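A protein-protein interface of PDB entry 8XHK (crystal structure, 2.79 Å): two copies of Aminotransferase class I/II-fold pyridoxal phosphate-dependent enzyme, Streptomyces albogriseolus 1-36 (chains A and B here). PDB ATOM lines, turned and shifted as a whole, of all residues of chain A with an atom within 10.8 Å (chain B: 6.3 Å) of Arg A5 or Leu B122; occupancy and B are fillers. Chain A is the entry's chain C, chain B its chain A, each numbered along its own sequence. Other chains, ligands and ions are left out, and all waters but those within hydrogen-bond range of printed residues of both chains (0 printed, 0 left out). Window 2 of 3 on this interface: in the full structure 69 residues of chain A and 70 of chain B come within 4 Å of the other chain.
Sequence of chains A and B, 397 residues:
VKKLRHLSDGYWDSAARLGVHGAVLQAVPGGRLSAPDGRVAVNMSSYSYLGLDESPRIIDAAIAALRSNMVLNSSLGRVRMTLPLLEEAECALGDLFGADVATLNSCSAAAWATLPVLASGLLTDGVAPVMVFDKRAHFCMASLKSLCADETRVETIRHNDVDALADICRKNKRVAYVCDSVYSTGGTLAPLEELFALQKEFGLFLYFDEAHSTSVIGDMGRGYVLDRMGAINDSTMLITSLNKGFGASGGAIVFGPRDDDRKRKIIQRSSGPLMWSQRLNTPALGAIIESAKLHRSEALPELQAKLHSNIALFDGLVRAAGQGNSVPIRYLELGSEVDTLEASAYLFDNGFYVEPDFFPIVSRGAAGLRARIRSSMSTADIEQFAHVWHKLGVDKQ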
ATOM      1  N   LYS A   3      21.872  12.531 -18.923  1.00  0.00           N
ATOM      2  CA  LYS A   3      20.581  11.977 -19.319  1.00  0.00           C
ATOM      3  C   LYS A   3      20.104  10.969 -18.282  1.00  0.00           C
ATOM      4  O   LYS A   3      18.904  10.847 -18.031  1.00  0.00           O
ATOM      5  CB  LYS A   3      20.680  11.322 -20.702  1.00  0.00           C
ATOM      6  CG  LYS A   3      19.391  11.359 -21.524  1.00  0.00           C
ATOM      7  CD  LYS A   3      18.374  10.319 -21.069  1.00  0.00           C
ATOM      8  CE  LYS A   3      18.973   8.921 -21.066  1.00  0.00           C
ATOM      9  NZ  LYS A   3      17.962   7.880 -20.727  1.00  0.00           N
ATOM     10  N   LEU A   4      21.058  10.258 -17.671  1.00  0.00           N
ATOM     11  CA  LEU A   4      20.738   9.252 -16.662  1.00  0.00           C
ATOM     12  C   LEU A   4      19.897   9.810 -15.520  1.00  0.00           C
ATOM     13  O   LEU A   4      19.282   9.035 -14.778  1.00  0.00           O
ATOM     14  CB  LEU A   4      22.031   8.637 -16.115  1.00  0.00           C
ATOM     15  CG  LEU A   4      23.294   9.504 -16.119  1.00  0.00           C
ATOM     16  CD1 LEU A   4      23.179  10.693 -15.170  1.00  0.00           C
ATOM     17  CD2 LEU A   4      24.512   8.659 -15.778  1.00  0.00           C
ATOM     18  N   ARG A   5      19.853  11.135 -15.369  1.00  0.00           N
ATOM     19  CA  ARG A   5      18.966  11.773 -14.405  1.00  0.00           C
ATOM     20  C   ARG A   5      17.493  11.573 -14.739  1.00  0.00           C
ATOM     21  O   ARG A   5      16.641  11.897 -13.904  1.00  0.00           O
ATOM     22  CB  ARG A   5      19.267  13.270 -14.329  1.00  0.00           C
ATOM     23  CG  ARG A   5      20.686  13.606 -13.913  1.00  0.00           C
ATOM     24  CD  ARG A   5      20.951  15.092 -14.074  1.00  0.00           C
ATOM     25  NE  ARG A   5      19.892  15.895 -13.474  1.00  0.00           N
ATOM     26  CZ  ARG A   5      19.901  16.333 -12.222  1.00  0.00           C
ATOM     27  NH1 ARG A   5      20.906  16.067 -11.404  1.00  0.00           N
ATOM     28  NH2 ARG A   5      18.878  17.060 -11.782  1.00  0.00           N
ATOM     29  N   HIS A   6      17.181  11.058 -15.931  1.00  0.00           N
ATOM     30  CA  HIS A   6      15.789  10.894 -16.342  1.00  0.00           C
ATOM     31  C   HIS A   6      15.022  10.015 -15.360  1.00  0.00           C
ATOM     32  O   HIS A   6      13.942  10.388 -14.887  1.00  0.00           O
ATOM     33  CB  HIS A   6      15.728  10.309 -17.757  1.00  0.00           C
ATOM     34  CG  HIS A   6      16.224   8.898 -17.849  1.00  0.00           C
ATOM     35  ND1 HIS A   6      17.532   8.550 -17.583  1.00  0.00           N
ATOM     36  CD2 HIS A   6      15.584   7.746 -18.156  1.00  0.00           C
ATOM     37  CE1 HIS A   6      17.676   7.245 -17.730  1.00  0.00           C
ATOM     38  NE2 HIS A   6      16.509   6.733 -18.080  1.00  0.00           N
ATOM     39  N   LEU A   7      15.573   8.844 -15.033  1.00  0.00           N
ATOM     40  CA  LEU A   7      14.929   7.913 -14.118  1.00  0.00           C
ATOM     41  C   LEU A   7      15.379   8.096 -12.678  1.00  0.00           C
ATOM     42  O   LEU A   7      14.630   7.740 -11.763  1.00  0.00           O
ATOM     43  CB  LEU A   7      15.196   6.467 -14.557  1.00  0.00           C
ATOM     44  CG  LEU A   7      13.979   5.597 -14.883  1.00  0.00           C
ATOM     45  CD1 LEU A   7      13.071   5.458 -13.671  1.00  0.00           C
ATOM     46  CD2 LEU A   7      13.214   6.161 -16.071  1.00  0.00           C
ATOM     47  N   SER A   8      16.575   8.649 -12.459  1.00  0.00           N
ATOM     48  CA  SER A   8      17.068   8.853 -11.099  1.00  0.00           C
ATOM     49  C   SER A   8      16.114   9.731 -10.301  1.00  0.00           C
ATOM     50  O   SER A   8      15.566   9.308  -9.276  1.00  0.00           O
ATOM     51  CB  SER A   8      18.468   9.468 -11.133  1.00  0.00           C
ATOM     52  OG  SER A   8      18.408  10.854 -11.414  1.00  0.00           O
ATOM     53  N   ASP A   9      15.891  10.963 -10.767  1.00  0.00           N
ATOM     54  CA  ASP A   9      14.915  11.838 -10.127  1.00  0.00           C
ATOM     55  C   ASP A   9      13.493  11.315 -10.274  1.00  0.00           C
ATOM     56  O   ASP A   9      12.603  11.764  -9.545  1.00  0.00           O
ATOM     57  CB  ASP A   9      15.008  13.256 -10.698  1.00  0.00           C
ATOM     58  CG  ASP A   9      16.345  13.916 -10.412  1.00  0.00           C
ATOM     59  OD1 ASP A   9      17.325  13.192 -10.140  1.00  0.00           O
ATOM     60  OD2 ASP A   9      16.413  15.163 -10.452  1.00  0.00           O
ATOM     61  N   GLY A  10      13.260  10.385 -11.204  1.00  0.00           N
ATOM     62  CA  GLY A  10      11.943   9.785 -11.319  1.00  0.00           C
ATOM     63  C   GLY A  10      11.542   9.017 -10.075  1.00  0.00           C
ATOM     64  O   GLY A  10      10.366   8.987  -9.703  1.00  0.00           O
ATOM     65  N   TYR A  11      12.514   8.383  -9.411  1.00  0.00           N
ATOM     66  CA  TYR A  11      12.219   7.701  -8.154  1.00  0.00           C
ATOM     67  C   TYR A  11      11.976   8.702  -7.032  1.00  0.00           C
ATOM     68  O   TYR A  11      11.096   8.493  -6.189  1.00  0.00           O
ATOM     69  CB  TYR A  11      13.359   6.753  -7.774  1.00  0.00           C
ATOM     70  CG  TYR A  11      13.738   5.752  -8.841  1.00  0.00           C
ATOM     71  CD1 TYR A  11      12.872   4.730  -9.205  1.00  0.00           C
ATOM     72  CD2 TYR A  11      14.976   5.815  -9.465  1.00  0.00           C
ATOM     73  CE1 TYR A  11      13.223   3.808 -10.175  1.00  0.00           C
ATOM     74  CE2 TYR A  11      15.335   4.903 -10.435  1.00  0.00           C
ATOM     75  CZ  TYR A  11      14.456   3.901 -10.786  1.00  0.00           C
ATOM     76  OH  TYR A  11      14.815   2.989 -11.752  1.00  0.00           O
ATOM     77  N   TRP A  12      12.756   9.790  -7.003  1.00  0.00           N
ATOM     78  CA  TRP A  12      12.600  10.804  -5.964  1.00  0.00           C
ATOM     79  C   TRP A  12      11.173  11.332  -5.909  1.00  0.00           C
ATOM     80  O   TRP A  12      10.616  11.529  -4.822  1.00  0.00           O
ATOM     81  CB  TRP A  12      13.574  11.961  -6.203  1.00  0.00           C
ATOM     82  CG  TRP A  12      15.025  11.639  -5.981  1.00  0.00           C
ATOM     83  CD1 TRP A  12      15.903  11.140  -6.898  1.00  0.00           C
ATOM     84  CD2 TRP A  12      15.771  11.824  -4.771  1.00  0.00           C
ATOM     85  NE1 TRP A  12      17.146  10.994  -6.332  1.00  0.00           N
ATOM     86  CE2 TRP A  12      17.092  11.406  -5.027  1.00  0.00           C
ATOM     87  CE3 TRP A  12      15.448  12.298  -3.496  1.00  0.00           C
ATOM     88  CZ2 TRP A  12      18.090  11.447  -4.056  1.00  0.00           C
ATOM     89  CZ3 TRP A  12      16.442  12.338  -2.534  1.00  0.00           C
ATOM     90  CH2 TRP A  12      17.745  11.913  -2.818  1.00  0.00           C
ATOM     91  N   ASP A  13      10.566  11.575  -7.073  1.00  0.00           N
ATOM     92  CA  ASP A  13       9.181  12.036  -7.101  1.00  0.00           C
ATOM     93  C   ASP A  13       8.226  10.938  -6.648  1.00  0.00           C
ATOM     94  O   ASP A  13       7.217  11.219  -5.991  1.00  0.00           O
ATOM     95  CB  ASP A  13       8.817  12.528  -8.502  1.00  0.00           C
ATOM     96  CG  ASP A  13       9.258  13.959  -8.750  1.00  0.00           C
ATOM     97  OD1 ASP A  13       8.969  14.828  -7.900  1.00  0.00           O
ATOM     98  OD2 ASP A  13       9.899  14.216  -9.792  1.00  0.00           O
ATOM     99  N   PHE A 359      18.281   4.415  -6.008  1.00  0.00           N
ATOM    100  CA  PHE A 359      19.102   5.135  -6.966  1.00  0.00           C
ATOM    101  C   PHE A 359      18.801   6.630  -6.876  1.00  0.00           C
ATOM    102  O   PHE A 359      17.630   7.022  -6.795  1.00  0.00           O
ATOM    103  CB  PHE A 359      18.822   4.607  -8.377  1.00  0.00           C
ATOM    104  CG  PHE A 359      19.803   5.069  -9.421  1.00  0.00           C
ATOM    105  CD1 PHE A 359      21.119   4.637  -9.397  1.00  0.00           C
ATOM    106  CD2 PHE A 359      19.395   5.903 -10.450  1.00  0.00           C
ATOM    107  CE1 PHE A 359      22.018   5.054 -10.365  1.00  0.00           C
ATOM    108  CE2 PHE A 359      20.287   6.319 -11.421  1.00  0.00           C
ATOM    109  CZ  PHE A 359      21.601   5.894 -11.378  1.00  0.00           C
ATOM    110  N   PRO A 360      19.825   7.501  -6.887  1.00  0.00           N
ATOM    111  CA  PRO A 360      21.253   7.206  -7.045  1.00  0.00           C
ATOM    112  C   PRO A 360      22.025   7.002  -5.739  1.00  0.00           C
ATOM    113  O   PRO A 360      23.243   6.829  -5.798  1.00  0.00           O
ATOM    114  CB  PRO A 360      21.767   8.449  -7.766  1.00  0.00           C
ATOM    115  CG  PRO A 360      20.939   9.548  -7.186  1.00  0.00           C
ATOM    116  CD  PRO A 360      19.575   8.953  -6.901  1.00  0.00           C
ATOM    117  N   ARG A 364      21.453   0.657  -8.944  1.00  0.00           N
ATOM    118  CA  ARG A 364      20.172   0.252  -9.506  1.00  0.00           C
ATOM    119  C   ARG A 364      19.906  -1.221  -9.227  1.00  0.00           C
ATOM    120  O   ARG A 364      20.818  -2.053  -9.256  1.00  0.00           O
ATOM    121  CB  ARG A 364      20.145   0.518 -11.011  1.00  0.00           C
ATOM    122  CG  ARG A 364      19.412   1.792 -11.402  1.00  0.00           C
ATOM    123  CD  ARG A 364      20.081   2.472 -12.586  1.00  0.00           C
ATOM    124  NE  ARG A 364      20.301   1.556 -13.698  1.00  0.00           N
ATOM    125  CZ  ARG A 364      20.950   1.873 -14.811  1.00  0.00           C
ATOM    126  NH1 ARG A 364      21.456   3.080 -14.995  1.00  0.00           N
ATOM    127  NH2 ARG A 364      21.094   0.954 -15.762  1.00  0.00           N
ATOM    128  N   VAL B 117      27.782  22.455  -7.803  1.00  0.00           N
ATOM    129  CA  VAL B 117      26.605  22.154  -8.613  1.00  0.00           C
ATOM    130  C   VAL B 117      26.441  23.187  -9.722  1.00  0.00           C
ATOM    131  O   VAL B 117      26.103  22.845 -10.861  1.00  0.00           O
ATOM    132  CB  VAL B 117      25.353  22.075  -7.721  1.00  0.00           C
ATOM    133  CG1 VAL B 117      24.128  21.729  -8.552  1.00  0.00           C
ATOM    134  CG2 VAL B 117      25.557  21.056  -6.610  1.00  0.00           C
ATOM    135  N   LEU B 118      26.679  24.463  -9.407  1.00  0.00           N
ATOM    136  CA  LEU B 118      26.568  25.511 -10.417  1.00  0.00           C
ATOM    137  C   LEU B 118      27.648  25.367 -11.482  1.00  0.00           C
ATOM    138  O   LEU B 118      27.403  25.633 -12.664  1.00  0.00           O
ATOM    139  CB  LEU B 118      26.644  26.885  -9.753  1.00  0.00           C
ATOM    140  CG  LEU B 118      26.581  28.104 -10.672  1.00  0.00           C
ATOM    141  CD1 LEU B 118      25.248  28.159 -11.401  1.00  0.00           C
ATOM    142  CD2 LEU B 118      26.821  29.383  -9.883  1.00  0.00           C
ATOM    143  N   ALA B 119      28.849  24.943 -11.081  1.00  0.00           N
ATOM    144  CA  ALA B 119      29.938  24.762 -12.033  1.00  0.00           C
ATOM    145  C   ALA B 119      29.691  23.601 -12.986  1.00  0.00           C
ATOM    146  O   ALA B 119      30.274  23.576 -14.075  1.00  0.00           O
ATOM    147  CB  ALA B 119      31.255  24.548 -11.287  1.00  0.00           C
ATOM    148  N   SER B 120      28.847  22.645 -12.606  1.00  0.00           N
ATOM    149  CA  SER B 120      28.547  21.496 -13.452  1.00  0.00           C
ATOM    150  C   SER B 120      27.497  21.795 -14.513  1.00  0.00           C
ATOM    151  O   SER B 120      27.176  20.907 -15.310  1.00  0.00           O
ATOM    152  CB  SER B 120      28.081  20.318 -12.593  1.00  0.00           C
ATOM    153  OG  SER B 120      26.872  20.623 -11.919  1.00  0.00           O
ATOM    154  N   GLY B 121      26.953  23.009 -14.545  1.00  0.00           N
ATOM    155  CA  GLY B 121      25.914  23.347 -15.491  1.00  0.00           C
ATOM    156  C   GLY B 121      24.541  22.808 -15.159  1.00  0.00           C
ATOM    157  O   GLY B 121      23.587  23.108 -15.887  1.00  0.00           O
ATOM    158  N   LEU B 122      24.406  22.027 -14.084  1.00  0.00           N
ATOM    159  CA  LEU B 122      23.106  21.494 -13.697  1.00  0.00           C
ATOM    160  C   LEU B 122      22.106  22.591 -13.357  1.00  0.00           C
ATOM    161  O   LEU B 122      20.897  22.336 -13.368  1.00  0.00           O
ATOM    162  CB  LEU B 122      23.264  20.543 -12.509  1.00  0.00           C
ATOM    163  CG  LEU B 122      23.750  19.130 -12.832  1.00  0.00           C
ATOM    164  CD1 LEU B 122      24.283  18.441 -11.585  1.00  0.00           C
ATOM    165  CD2 LEU B 122      22.620  18.321 -13.444  1.00  0.00           C
ATOM    166  N   LEU B 123      22.577  23.798 -13.059  1.00  0.00           N
ATOM    167  CA  LEU B 123      21.710  24.933 -12.781  1.00  0.00           C
ATOM    168  C   LEU B 123      21.626  25.909 -13.946  1.00  0.00           C
ATOM    169  O   LEU B 123      20.928  26.922 -13.838  1.00  0.00           O
ATOM    170  CB  LEU B 123      22.189  25.667 -11.525  1.00  0.00           C
ATOM    171  CG  LEU B 123      22.231  24.840 -10.240  1.00  0.00           C
ATOM    172  CD1 LEU B 123      22.829  25.648  -9.104  1.00  0.00           C
ATOM    173  CD2 LEU B 123      20.839  24.345  -9.874  1.00  0.00           C
ATOM    174  N   THR B 124      22.316  25.632 -15.053  1.00  0.00           N
ATOM    175  CA  THR B 124      22.333  26.516 -16.215  1.00  0.00           C
ATOM    176  C   THR B 124      22.053  25.707 -17.486  1.00  0.00           C
ATOM    177  O   THR B 124      22.857  25.663 -18.416  1.00  0.00           O
ATOM    178  CB  THR B 124      23.660  27.266 -16.321  1.00  0.00           C
ATOM    179  OG1 THR B 124      24.746  26.356 -16.104  1.00  0.00           O
ATOM    180  CG2 THR B 124      23.723  28.383 -15.292  1.00  0.00           C
ATOM    181  N   ASP B 125      20.891  25.051 -17.508  1.00  0.00           N
ATOM    182  CA  ASP B 125      20.360  24.391 -18.703  1.00  0.00           C
ATOM    183  C   ASP B 125      21.277  23.279 -19.210  1.00  0.00           C
ATOM    184  O   ASP B 125      21.261  22.941 -20.396  1.00  0.00           O
ATOM    185  CB  ASP B 125      20.093  25.406 -19.819  1.00  0.00           C
ATOM    186  CG  ASP B 125      19.381  26.649 -19.320  1.00  0.00           C
ATOM    187  OD1 ASP B 125      18.481  26.518 -18.462  1.00  0.00           O
ATOM    188  OD2 ASP B 125      19.726  27.759 -19.779  1.00  0.00           O
ATOM    189  N   GLY B 126      22.077  22.693 -18.320  1.00  0.00           N
ATOM    190  CA  GLY B 126      23.010  21.655 -18.701  1.00  0.00           C
ATOM    191  C   GLY B 126      24.314  22.142 -19.292  1.00  0.00           C
ATOM    192  O   GLY B 126      25.241  21.337 -19.452  1.00  0.00           O
ATOM    193  N   VAL B 127      24.422  23.426 -19.622  1.00  0.00           N
ATOM    194  CA  VAL B 127      25.639  23.990 -20.196  1.00  0.00           C
ATOM    195  C   VAL B 127      26.541  24.421 -19.046  1.00  0.00           C
ATOM    196  O   VAL B 127      26.214  25.350 -18.303  1.00  0.00           O
ATOM    197  CB  VAL B 127      25.330  25.166 -21.129  1.00  0.00           C
ATOM    198  CG1 VAL B 127      26.615  25.708 -21.740  1.00  0.00           C
ATOM    199  CG2 VAL B 127      24.351  24.742 -22.212  1.00  0.00           C
ATOM    200  N   ALA B 128      27.680  23.744 -18.900  1.00  0.00           N
ATOM    201  CA  ALA B 128      28.638  24.058 -17.848  1.00  0.00           C
ATOM    202  C   ALA B 128      29.194  25.461 -18.051  1.00  0.00           C
ATOM    203  O   ALA B 128      29.892  25.716 -19.041  1.00  0.00           O
ATOM    204  CB  ALA B 128      29.770  23.028 -17.825  1.00  0.00           C
ATOM    205  N   PRO B 129      28.913  26.391 -17.144  1.00  0.00           N
ATOM    206  CA  PRO B 129      29.358  27.772 -17.338  1.00  0.00           C
ATOM    207  C   PRO B 129      30.810  27.965 -16.928  1.00  0.00           C
ATOM    208  O   PRO B 129      31.415  27.135 -16.247  1.00  0.00           O
ATOM    209  CB  PRO B 129      28.423  28.567 -16.424  1.00  0.00           C
ATOM    210  CG  PRO B 129      28.152  27.624 -15.298  1.00  0.00           C
ATOM    211  CD  PRO B 129      28.140  26.233 -15.900  1.00  0.00           C
ATOM    212  N   LYS B 265      15.561  21.098  -5.825  1.00  0.00           N
ATOM    213  CA  LYS B 265      15.592  19.650  -6.005  1.00  0.00           C
ATOM    214  C   LYS B 265      16.889  19.185  -6.654  1.00  0.00           C
ATOM    215  O   LYS B 265      17.363  18.083  -6.358  1.00  0.00           O
ATOM    216  CB  LYS B 265      14.389  19.195  -6.831  1.00  0.00           C
ATOM    217  CG  LYS B 265      13.059  19.289  -6.098  1.00  0.00           C
ATOM    218  CD  LYS B 265      11.928  18.717  -6.935  1.00  0.00           C
ATOM    219  CE  LYS B 265      10.618  18.700  -6.160  1.00  0.00           C
ATOM    220  NZ  LYS B 265       9.508  18.107  -6.957  1.00  0.00           N
ATOM    221  N   ILE B 266      17.475  19.999  -7.533  1.00  0.00           N
ATOM    222  CA  ILE B 266      18.735  19.614  -8.163  1.00  0.00           C
ATOM    223  C   ILE B 266      19.852  19.553  -7.129  1.00  0.00           C
ATOM    224  O   ILE B 266      20.701  18.655  -7.165  1.00  0.00           O
ATOM    225  CB  ILE B 266      19.076  20.573  -9.318  1.00  0.00           C
ATOM    226  CG1 ILE B 266      18.152  20.322 -10.510  1.00  0.00           C
ATOM    227  CG2 ILE B 266      20.530  20.422  -9.737  1.00  0.00           C
ATOM    228  CD1 ILE B 266      18.353  21.290 -11.651  1.00  0.00           C
ATOM    229  N   ARG B 269      19.239  16.570  -4.432  1.00  0.00           N
ATOM    230  CA  ARG B 269      19.560  15.272  -5.006  1.00  0.00           C
ATOM    231  C   ARG B 269      20.977  15.208  -5.559  1.00  0.00           C
ATOM    232  O   ARG B 269      21.385  14.155  -6.060  1.00  0.00           O
ATOM    233  CB  ARG B 269      18.541  14.930  -6.099  1.00  0.00           C
ATOM    234  CG  ARG B 269      17.110  14.917  -5.574  1.00  0.00           C
ATOM    235  CD  ARG B 269      16.068  15.043  -6.673  1.00  0.00           C
ATOM    236  NE  ARG B 269      14.726  15.159  -6.111  1.00  0.00           N
ATOM    237  CZ  ARG B 269      13.620  15.334  -6.823  1.00  0.00           C
ATOM    238  NH1 ARG B 269      13.655  15.421  -8.142  1.00  0.00           N
ATOM    239  NH2 ARG B 269      12.451  15.423  -6.195  1.00  0.00           N
ATOM    240  N   SER B 270      21.732  16.297  -5.475  1.00  0.00           N
ATOM    241  CA  SER B 270      23.135  16.299  -5.854  1.00  0.00           C
ATOM    242  C   SER B 270      24.005  15.953  -4.652  1.00  0.00           C
ATOM    243  O   SER B 270      23.581  16.038  -3.497  1.00  0.00           O
ATOM    244  CB  SER B 270      23.544  17.659  -6.420  1.00  0.00           C
ATOM    245  OG  SER B 270      24.947  17.736  -6.599  1.00  0.00           O
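No position is printed for both chains. Of the 6 pairs that touch across the chains among the printed residues, none has its exchanged pair printed and touching as well.
Of the 17 printed residues of chain B, 4 touch a printed residue of chain A. Printed residues of chain B that touch a printed residue of chain A: Leu B122, Lys B265, Ile B266 and Arg B269. Hydrophobic or aromatic side chains of chain B that line the printed part of chain A: Leu B122 and Ile B266. Of the 14 printed residues of chain A, 4 touch a printed residue of chain B. Hydrophobic or aromatic side chains of chain A that line the printed part of chain B: Trp A12.
The backbone carbonyl oxygen (O) of Arg A5 sits close to the side-chain hydroxyl (OG) of Ser A8 (3.2 Å). The guanidinium group (NH2) of Arg A5 is in salt-bridge range of the side-chain carboxylate (OD2) of Asp A9, 3.4 Å away. The side-chain carboxylate (OD1) of Asp A9 lies within hydrogen-bond range of the side-chain hydroxyl (OG) of Ser A8.
Among the printed residues, pairs that only touch across the chains: Arg A5 with Leu B122 (3.5 Å), Arg A5 with Ile B266 (3.6 Å) and Trp A12 with Arg B269 (3.4 Å).
The guanidinium group (NH1) of Arg B269 is in salt-bridge range of the side-chain carboxylate (OD2) of Asp A9 (3.6 Å). The side-chain carboxylate (OD1) of Asp A13 lies within salt-bridge range of the side-chain amino group (NZ) of Lys B265, at 3.5 Å. OD1 of Asp A13 lies within salt-bridge range of NH2 of Arg B269.
Of chain B, only Leu B122 and Ile B266 come within 4 Å of Arg A5. No residue of chain A comes within 4 Å of Val B117. No residue of chain A comes within 4 Å of Ser B120. No residue of chain A comes within 4 Å of Gly B121. No residue of chain A comes within 4 Å of Leu B123. No residue of chain A comes within 4 Å of Thr B124. No residue of chain A comes within 4 Å of Gly B126. Of the printed residues of chain A, Ile B266 touches Arg A5 (3.6 Å). Printed residues of chain A within 4 Å of Arg B269: Asp A9 (3.6 Å), Trp A12 (3.4 Å) and Asp A13 (3.9 Å). Of the printed residues of chain B, Asp A9 touches Arg B269. Of the printed residues of chain B, Trp A12 touches Arg B269 (3.4 Å). Of the printed residues of chain A, Lys B265 touches Asp A13 (3.5 Å). Asp B125 touches none of the printed residues of chain A. Leu A7 touches none of the printed residues of chain B. The nearest printed residue of chain B that does not touch Arg A5 is Arg B269 (5.7 Å). The nearest printed residue of chain B that does not touch Asp A13 is Ile B266 (9.8 Å).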
